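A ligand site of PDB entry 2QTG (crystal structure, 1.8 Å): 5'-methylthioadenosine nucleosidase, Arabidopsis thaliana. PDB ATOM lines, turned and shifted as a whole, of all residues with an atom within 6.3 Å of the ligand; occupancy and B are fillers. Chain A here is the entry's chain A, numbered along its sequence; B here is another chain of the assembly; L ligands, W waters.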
ATOM      1  N   ALA A  34     -15.403 -22.373 -21.131  1.00  0.00           N
ATOM      2  CA  ALA A  34     -15.335 -20.956 -20.706  1.00  0.00           C
ATOM      3  C   ALA A  34     -14.884 -20.747 -19.230  1.00  0.00           C
ATOM      4  O   ALA A  34     -14.108 -19.828 -18.942  1.00  0.00           O
ATOM      5  CB  ALA A  34     -16.655 -20.286 -20.928  1.00  0.00           C
ATOM      6  N   MET A  35     -15.363 -21.618 -18.347  1.00  0.00           N
ATOM      7  CA  MET A  35     -15.038 -21.552 -16.916  1.00  0.00           C
ATOM      8  C   MET A  35     -14.202 -22.733 -16.422  1.00  0.00           C
ATOM      9  O   MET A  35     -14.519 -23.901 -16.710  1.00  0.00           O
ATOM     10  CB  MET A  35     -16.319 -21.453 -16.084  1.00  0.00           C
ATOM     11  CG  MET A  35     -17.240 -20.306 -16.532  1.00  0.00           C
ATOM     12  SD  MET A  35     -18.458 -19.869 -15.267  1.00  0.00           S
ATOM     13  CE  MET A  35     -19.501 -21.321 -15.381  1.00  0.00           C
ATOM     14  N   GLU A  38     -15.942 -25.831 -15.117  1.00  0.00           N
ATOM     15  CA  GLU A  38     -16.486 -26.709 -16.165  1.00  0.00           C
ATOM     16  C   GLU A  38     -15.353 -27.591 -16.775  1.00  0.00           C
ATOM     17  O   GLU A  38     -15.626 -28.673 -17.320  1.00  0.00           O
ATOM     18  CB  GLU A  38     -17.175 -25.879 -17.282  1.00  0.00           C
ATOM     19  CG  GLU A  38     -18.447 -25.017 -16.947  1.00  0.00           C
ATOM     20  CD  GLU A  38     -18.781 -23.902 -18.038  1.00  0.00           C
ATOM     21  OE1 GLU A  38     -17.858 -23.377 -18.714  1.00  0.00           O
ATOM     22  OE2 GLU A  38     -19.960 -23.541 -18.227  1.00  0.00           O
ATOM     23  N   ASP A  88     -13.496 -15.898 -13.935  1.00  0.00           N
ATOM     24  CA  ASP A  88     -13.412 -16.522 -15.275  1.00  0.00           C
ATOM     25  C   ASP A  88     -13.876 -15.556 -16.372  1.00  0.00           C
ATOM     26  O   ASP A  88     -14.939 -14.933 -16.279  1.00  0.00           O
ATOM     27  CB  ASP A  88     -14.217 -17.835 -15.412  1.00  0.00           C
ATOM     28  CG  ASP A  88     -13.555 -19.010 -14.694  1.00  0.00           C
ATOM     29  OD1 ASP A  88     -12.513 -19.532 -15.124  1.00  0.00           O
ATOM     30  OD2 ASP A  88     -14.127 -19.413 -13.688  1.00  0.00           O
ATOM     31  N   VAL A  90     -15.573 -15.123 -19.031  1.00  0.00           N
ATOM     32  CA  VAL A  90     -16.763 -15.598 -19.766  1.00  0.00           C
ATOM     33  C   VAL A  90     -17.145 -14.622 -20.893  1.00  0.00           C
ATOM     34  O   VAL A  90     -16.645 -13.481 -20.959  1.00  0.00           O
ATOM     35  CB  VAL A  90     -17.998 -15.794 -18.812  1.00  0.00           C
ATOM     36  CG1 VAL A  90     -17.773 -16.918 -17.821  1.00  0.00           C
ATOM     37  CG2 VAL A  90     -18.351 -14.473 -18.038  1.00  0.00           C
ATOM     38  N   GLY A  91     -17.998 -15.089 -21.811  1.00  0.00           N
ATOM     39  CA  GLY A  91     -18.549 -14.213 -22.844  1.00  0.00           C
ATOM     40  C   GLY A  91     -17.884 -14.365 -24.200  1.00  0.00           C
ATOM     41  O   GLY A  91     -16.911 -15.106 -24.360  1.00  0.00           O
ATOM     42  N   GLY A 115     -19.912 -26.835 -21.959  1.00  0.00           N
ATOM     43  CA  GLY A 115     -20.154 -26.023 -20.770  1.00  0.00           C
ATOM     44  C   GLY A 115     -21.606 -26.011 -20.316  1.00  0.00           C
ATOM     45  O   GLY A 115     -22.464 -26.713 -20.884  1.00  0.00           O
ATOM     46  N   THR A 116     -21.869 -25.213 -19.303  1.00  0.00           N
ATOM     47  CA  THR A 116     -23.233 -25.044 -18.753  1.00  0.00           C
ATOM     48  C   THR A 116     -24.055 -23.994 -19.550  1.00  0.00           C
ATOM     49  O   THR A 116     -23.498 -23.156 -20.276  1.00  0.00           O
ATOM     50  CB  THR A 116     -23.172 -24.717 -17.224  1.00  0.00           C
ATOM     51  OG1 THR A 116     -22.391 -23.506 -17.014  1.00  0.00           O
ATOM     52  CG2 THR A 116     -22.542 -25.845 -16.469  1.00  0.00           C
ATOM     53  N   CYS A 117     -25.366 -24.066 -19.417  1.00  0.00           N
ATOM     54  CA  CYS A 117     -26.249 -23.167 -20.095  1.00  0.00           C
ATOM     55  C   CYS A 117     -27.595 -23.087 -19.391  1.00  0.00           C
ATOM     56  O   CYS A 117     -27.900 -23.940 -18.509  1.00  0.00           O
ATOM     57  CB  CYS A 117     -26.471 -23.658 -21.556  1.00  0.00           C
ATOM     58  SG  CYS A 117     -27.385 -25.216 -21.672  1.00  0.00           S
ATOM     59  N   GLY A 118     -28.391 -22.114 -19.816  1.00  0.00           N
ATOM     60  CA  GLY A 118     -29.825 -22.023 -19.533  1.00  0.00           C
ATOM     61  C   GLY A 118     -30.597 -22.949 -20.487  1.00  0.00           C
ATOM     62  O   GLY A 118     -30.135 -23.235 -21.617  1.00  0.00           O
ATOM     63  N   GLY A 119     -31.751 -23.411 -20.032  1.00  0.00           N
ATOM     64  CA  GLY A 119     -32.649 -24.198 -20.873  1.00  0.00           C
ATOM     65  C   GLY A 119     -34.084 -23.776 -20.648  1.00  0.00           C
ATOM     66  O   GLY A 119     -34.415 -23.210 -19.586  1.00  0.00           O
ATOM     67  N   GLY A 178     -25.690 -14.815 -26.121  1.00  0.00           N
ATOM     68  CA  GLY A 178     -25.545 -13.371 -25.919  1.00  0.00           C
ATOM     69  C   GLY A 178     -24.624 -13.079 -24.751  1.00  0.00           C
ATOM     70  O   GLY A 178     -24.337 -13.999 -23.991  1.00  0.00           O
ATOM     71  N   SER A 180     -25.017 -11.622 -21.864  1.00  0.00           N
ATOM     72  CA  SER A 180     -25.623 -11.372 -20.514  1.00  0.00           C
ATOM     73  C   SER A 180     -26.103 -12.676 -19.888  1.00  0.00           C
ATOM     74  O   SER A 180     -26.635 -13.515 -20.587  1.00  0.00           O
ATOM     75  CB  SER A 180     -26.756 -10.321 -20.581  1.00  0.00           C
ATOM     76  OG  SER A 180     -26.280  -9.095 -21.122  1.00  0.00           O
ATOM     77  N   LEU A 181     -25.841 -12.874 -18.593  1.00  0.00           N
ATOM     78  CA  LEU A 181     -26.313 -14.021 -17.848  1.00  0.00           C
ATOM     79  C   LEU A 181     -27.797 -13.940 -17.539  1.00  0.00           C
ATOM     80  O   LEU A 181     -28.501 -14.968 -17.489  1.00  0.00           O
ATOM     81  CB  LEU A 181     -25.495 -14.212 -16.549  1.00  0.00           C
ATOM     82  CG  LEU A 181     -26.016 -15.242 -15.541  1.00  0.00           C
ATOM     83  CD1 LEU A 181     -25.949 -16.665 -16.122  1.00  0.00           C
ATOM     84  CD2 LEU A 181     -25.172 -15.148 -14.263  1.00  0.00           C
ATOM     85  N   ASP A 182     -28.307 -12.741 -17.330  1.00  0.00           N
ATOM     86  CA  ASP A 182     -29.712 -12.586 -17.099  1.00  0.00           C
ATOM     87  C   ASP A 182     -30.438 -12.525 -18.441  1.00  0.00           C
ATOM     88  O   ASP A 182     -29.846 -12.753 -19.483  1.00  0.00           O
ATOM     89  CB  ASP A 182     -29.999 -11.383 -16.206  1.00  0.00           C
ATOM     90  CG  ASP A 182     -29.577 -10.073 -16.813  1.00  0.00           C
ATOM     91  OD1 ASP A 182     -29.084 -10.012 -17.970  1.00  0.00           O
ATOM     92  OD2 ASP A 182     -29.775  -9.080 -16.106  1.00  0.00           O
ATOM     93  N   LYS A 199     -29.509 -21.478 -23.912  1.00  0.00           N
ATOM     94  CA  LYS A 199     -29.080 -20.088 -23.754  1.00  0.00           C
ATOM     95  C   LYS A 199     -27.708 -20.052 -23.106  1.00  0.00           C
ATOM     96  O   LYS A 199     -27.490 -20.615 -22.014  1.00  0.00           O
ATOM     97  CB  LYS A 199     -30.107 -19.290 -22.931  1.00  0.00           C
ATOM     98  CG  LYS A 199     -29.722 -17.801 -22.712  1.00  0.00           C
ATOM     99  CD  LYS A 199     -30.537 -17.164 -21.573  1.00  0.00           C
ATOM    100  CE  LYS A 199     -30.176 -15.661 -21.441  1.00  0.00           C
ATOM    101  NZ  LYS A 199     -28.869 -15.485 -20.740  1.00  0.00           N
ATOM    102  N   ASP A 200     -26.765 -19.367 -23.758  1.00  0.00           N
ATOM    103  CA  ASP A 200     -25.425 -19.244 -23.179  1.00  0.00           C
ATOM    104  C   ASP A 200     -24.779 -17.908 -23.521  1.00  0.00           C
ATOM    105  O   ASP A 200     -25.442 -16.996 -24.083  1.00  0.00           O
ATOM    106  CB  ASP A 200     -24.540 -20.421 -23.603  1.00  0.00           C
ATOM    107  CG  ASP A 200     -23.981 -20.269 -25.019  1.00  0.00           C
ATOM    108  OD1 ASP A 200     -24.585 -19.525 -25.825  1.00  0.00           O
ATOM    109  OD2 ASP A 200     -22.948 -20.888 -25.314  1.00  0.00           O
ATOM    110  N   MET A 201     -23.490 -17.807 -23.250  1.00  0.00           N
ATOM    111  CA  MET A 201     -22.756 -16.560 -23.503  1.00  0.00           C
ATOM    112  C   MET A 201     -21.537 -16.710 -24.410  1.00  0.00           C
ATOM    113  O   MET A 201     -20.829 -15.714 -24.645  1.00  0.00           O
ATOM    114  CB  MET A 201     -22.362 -15.901 -22.162  1.00  0.00           C
ATOM    115  CG  MET A 201     -23.587 -15.499 -21.329  1.00  0.00           C
ATOM    116  SD  MET A 201     -23.189 -15.253 -19.556  1.00  0.00           S
ATOM    117  CE  MET A 201     -22.149 -13.801 -19.556  1.00  0.00           C
ATOM    118  N   GLU A 202     -21.291 -17.938 -24.920  1.00  0.00           N
ATOM    119  CA  GLU A 202     -20.157 -18.124 -25.824  1.00  0.00           C
ATOM    120  C   GLU A 202     -20.423 -18.814 -27.170  1.00  0.00           C
ATOM    121  O   GLU A 202     -19.667 -18.558 -28.112  1.00  0.00           O
ATOM    122  CB  GLU A 202     -19.001 -18.876 -25.162  1.00  0.00           C
ATOM    123  CG  GLU A 202     -18.388 -18.240 -23.910  1.00  0.00           C
ATOM    124  CD  GLU A 202     -19.180 -18.548 -22.622  1.00  0.00           C
ATOM    125  OE1 GLU A 202     -19.836 -19.605 -22.555  1.00  0.00           O
ATOM    126  OE2 GLU A 202     -19.075 -17.753 -21.674  1.00  0.00           O
ATOM    127  N   GLY A 203     -21.420 -19.701 -27.241  1.00  0.00           N
ATOM    128  CA  GLY A 203     -21.524 -20.699 -28.309  1.00  0.00           C
ATOM    129  C   GLY A 203     -21.422 -20.181 -29.728  1.00  0.00           C
ATOM    130  O   GLY A 203     -20.577 -20.648 -30.510  1.00  0.00           O
ATOM    131  N   LYS A 221     -23.849 -28.956 -24.202  1.00  0.00           N
ATOM    132  CA  LYS A 221     -24.371 -27.900 -23.309  1.00  0.00           C
ATOM    133  C   LYS A 221     -25.237 -28.514 -22.195  1.00  0.00           C
ATOM    134  O   LYS A 221     -26.299 -29.119 -22.461  1.00  0.00           O
ATOM    135  CB  LYS A 221     -25.124 -26.812 -24.086  1.00  0.00           C
ATOM    136  CG  LYS A 221     -24.206 -26.034 -25.076  1.00  0.00           C
ATOM    137  CD  LYS A 221     -23.249 -25.088 -24.331  1.00  0.00           C
ATOM    138  CE  LYS A 221     -22.063 -24.661 -25.234  1.00  0.00           C
ATOM    139  NZ  LYS A 221     -21.540 -23.302 -24.786  1.00  0.00           N
ATOM    140  N   THR A 224     -27.886 -26.028 -16.498  1.00  0.00           N
ATOM    141  CA  THR A 224     -27.854 -25.694 -15.066  1.00  0.00           C
ATOM    142  C   THR A 224     -29.007 -24.927 -14.491  1.00  0.00           C
ATOM    143  O   THR A 224     -29.181 -24.909 -13.289  1.00  0.00           O
ATOM    144  CB  THR A 224     -26.634 -24.852 -14.633  1.00  0.00           C
ATOM    145  OG1 THR A 224     -25.909 -24.302 -15.721  1.00  0.00           O
ATOM    146  CG2 THR A 224     -25.713 -25.603 -13.781  1.00  0.00           C
ATOM    147  N   ASP A 225     -29.701 -24.179 -15.325  1.00  0.00           N
ATOM    148  CA  ASP A 225     -30.890 -23.499 -14.847  1.00  0.00           C
ATOM    149  C   ASP A 225     -31.930 -23.456 -15.940  1.00  0.00           C
ATOM    150  O   ASP A 225     -31.602 -23.506 -17.120  1.00  0.00           O
ATOM    151  CB  ASP A 225     -30.590 -22.121 -14.279  1.00  0.00           C
ATOM    152  CG  ASP A 225     -30.409 -21.100 -15.322  1.00  0.00           C
ATOM    153  OD1 ASP A 225     -29.403 -21.190 -16.061  1.00  0.00           O
ATOM    154  OD2 ASP A 225     -31.269 -20.204 -15.392  1.00  0.00           O
ATOM    155  N   VAL A 227     -34.483 -21.253 -17.553  1.00  0.00           N
ATOM    156  CA  VAL A 227     -34.691 -19.810 -17.756  1.00  0.00           C
ATOM    157  C   VAL A 227     -36.169 -19.471 -17.523  1.00  0.00           C
ATOM    158  O   VAL A 227     -36.494 -18.396 -17.028  1.00  0.00           O
ATOM    159  CB  VAL A 227     -34.238 -19.381 -19.154  1.00  0.00           C
ATOM    160  CG1 VAL A 227     -34.586 -17.930 -19.376  1.00  0.00           C
ATOM    161  CG2 VAL A 227     -32.717 -19.617 -19.327  1.00  0.00           C
ATOM    162  N   ILE B 143     -23.880  -9.275 -16.121  1.00  0.00           N
ATOM    163  CA  ILE B 143     -23.703 -10.483 -15.339  1.00  0.00           C
ATOM    164  C   ILE B 143     -23.916 -10.167 -13.834  1.00  0.00           C
ATOM    165  O   ILE B 143     -22.974  -9.726 -13.164  1.00  0.00           O
ATOM    166  CB  ILE B 143     -22.297 -11.107 -15.524  1.00  0.00           C
ATOM    167  CG1 ILE B 143     -21.892 -11.046 -17.042  1.00  0.00           C
ATOM    168  CG2 ILE B 143     -22.275 -12.547 -14.951  1.00  0.00           C
ATOM    169  CD1 ILE B 143     -20.450 -11.260 -17.365  1.00  0.00           C
ATOM    170  N   ILE B 145     -23.693 -11.098 -10.879  1.00  0.00           N
ATOM    171  CA  ILE B 145     -22.919 -11.774  -9.822  1.00  0.00           C
ATOM    172  C   ILE B 145     -21.854 -10.732  -9.496  1.00  0.00           C
ATOM    173  O   ILE B 145     -21.299 -10.082 -10.421  1.00  0.00           O
ATOM    174  CB  ILE B 145     -22.246 -13.128 -10.299  1.00  0.00           C
ATOM    175  CG1 ILE B 145     -23.291 -14.192 -10.654  1.00  0.00           C
ATOM    176  CG2 ILE B 145     -21.393 -13.740  -9.207  1.00  0.00           C
ATOM    177  CD1 ILE B 145     -22.758 -15.358 -11.491  1.00  0.00           C
ATOM    178  N   PHE B 148     -18.315 -10.216 -11.397  1.00  0.00           N
ATOM    179  CA  PHE B 148     -18.569 -10.536 -12.793  1.00  0.00           C
ATOM    180  C   PHE B 148     -19.308  -9.330 -13.368  1.00  0.00           C
ATOM    181  O   PHE B 148     -19.126  -8.983 -14.528  1.00  0.00           O
ATOM    182  CB  PHE B 148     -19.465 -11.767 -12.918  1.00  0.00           C
ATOM    183  CG  PHE B 148     -18.735 -13.073 -12.946  1.00  0.00           C
ATOM    184  CD1 PHE B 148     -18.296 -13.621 -14.123  1.00  0.00           C
ATOM    185  CD2 PHE B 148     -18.545 -13.776 -11.800  1.00  0.00           C
ATOM    186  CE1 PHE B 148     -17.669 -14.822 -14.132  1.00  0.00           C
ATOM    187  CE2 PHE B 148     -17.892 -14.982 -11.824  1.00  0.00           C
ATOM    188  CZ  PHE B 148     -17.458 -15.490 -12.981  1.00  0.00           C
HETATM  189  C1  LIG L   1     -20.668 -16.727 -15.113  1.00  0.00           C
HETATM  190  S1  LIG L   1     -21.637 -16.258 -16.553  1.00  0.00           S
HETATM  191  C2  LIG L   1     -22.319 -17.856 -16.868  1.00  0.00           C
HETATM  192  C3  LIG L   1     -21.449 -18.841 -17.671  1.00  0.00           C
HETATM  193  O1  LIG L   1     -22.160 -20.101 -17.736  1.00  0.00           O
HETATM  194  C4  LIG L   1     -22.406 -18.955 -19.850  1.00  0.00           C
HETATM  195  O2  LIG L   1     -22.197 -19.439 -21.196  1.00  0.00           O
HETATM  196  C5  LIG L   1     -21.184 -18.436 -19.119  1.00  0.00           C
HETATM  197  O3  LIG L   1     -19.937 -19.055 -19.508  1.00  0.00           O
HETATM  198  C6  LIG L   1     -22.924 -20.132 -18.980  1.00  0.00           C
HETATM  199  N1  LIG L   1     -24.329 -19.973 -18.655  1.00  0.00           N
HETATM  200  C7  LIG L   1     -24.959 -20.570 -17.706  1.00  0.00           C
HETATM  201  C8  LIG L   1     -26.214 -20.423 -17.758  1.00  0.00           C
HETATM  202  C9  LIG L   1     -26.554 -19.356 -18.414  1.00  0.00           C
HETATM  203  C10 LIG L   1     -27.734 -18.690 -18.626  1.00  0.00           C
HETATM  204  N2  LIG L   1     -28.871 -19.007 -17.942  1.00  0.00           N
HETATM  205  N3  LIG L   1     -27.643 -17.676 -19.533  1.00  0.00           N
HETATM  206  C11 LIG L   1     -26.465 -17.377 -20.195  1.00  0.00           C
HETATM  207  N4  LIG L   1     -25.298 -18.060 -19.975  1.00  0.00           N
HETATM  208  C12 LIG L   1     -25.353 -19.083 -19.086  1.00  0.00           C
HETATM  209  O   HOH W   1     -19.907 -21.840 -19.944  1.00  0.00           O
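The side-chain amino group (NZ) of Lys 199 sits at hydrogen-bond distance from the backbone carbonyl oxygen (O) of Leu 181, at 3.3 Å.
The backbone carbonyl oxygen (O) of Asp 182 sits at hydrogen-bond distance from the side-chain amino group (NZ) of Lys 199.
O of Asp 225 sits at hydrogen-bond distance from N of Gly 119 (2.9 Å).
N of Met 35 is in hydrogen-bond range of OE1 of Glu 38, at 3.1 Å.
The backbone NH (N) of Gly 178 lies within hydrogen-bond range of the backbone carbonyl oxygen (O) of Asp 200, 3.0 Å away.
N of Gly 203 is in hydrogen-bond range of OD2 of Asp 200, at 2.7 Å.
The side-chain hydroxyl of Thr 116 sits at hydrogen-bond distance from the side-chain carboxylate of Glu 38.
The side-chain carboxylate (OD2) of Asp 200 is in salt-bridge range of the side-chain amino group (NZ) of Lys 221, 2.8 Å away.
A nitrogen (N3) of the ligand sits close to the backbone carbonyl oxygen of Leu 181 (3.5 Å).
Ala 34 touches the ligand (CB to O3, 3.8 Å).
Met 35 touches the ligand (CE to O1, 3.8 Å).
Val 90 touches the ligand.
Cys 117 touches the ligand (C to C8, 3.4 Å).
Gly 118 touches the ligand (N to C8, 3.4 Å).
Ser 180 touches the ligand.
Asp 200 touches the ligand (CA to N4, 3.4 Å).
CE1 of Phe 148 of chain B touches C1 of the ligand, 3.7 Å away.
Water W1 lies within hydrogen-bond range of OE2 of Glu 38, O3 of the ligand and OE1 of Glu 202.
The side-chain hydroxyl (OG1) of Thr 116 is in hydrogen-bond range of an oxygen (O1) of the ligand (3.5 Å).
OD1 of Asp 225 sits at hydrogen-bond distance from N2 of the ligand, at 2.9 Å.
O3 of the ligand lies within hydrogen-bond range of OE2 of Glu 202, at 2.7 Å.
A nitrogen (N3) of the ligand sits at hydrogen-bond distance from the side-chain amino group of Lys 199.
The backbone NH of Met 201 lies within hydrogen-bond range of an oxygen (O2) of the ligand.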
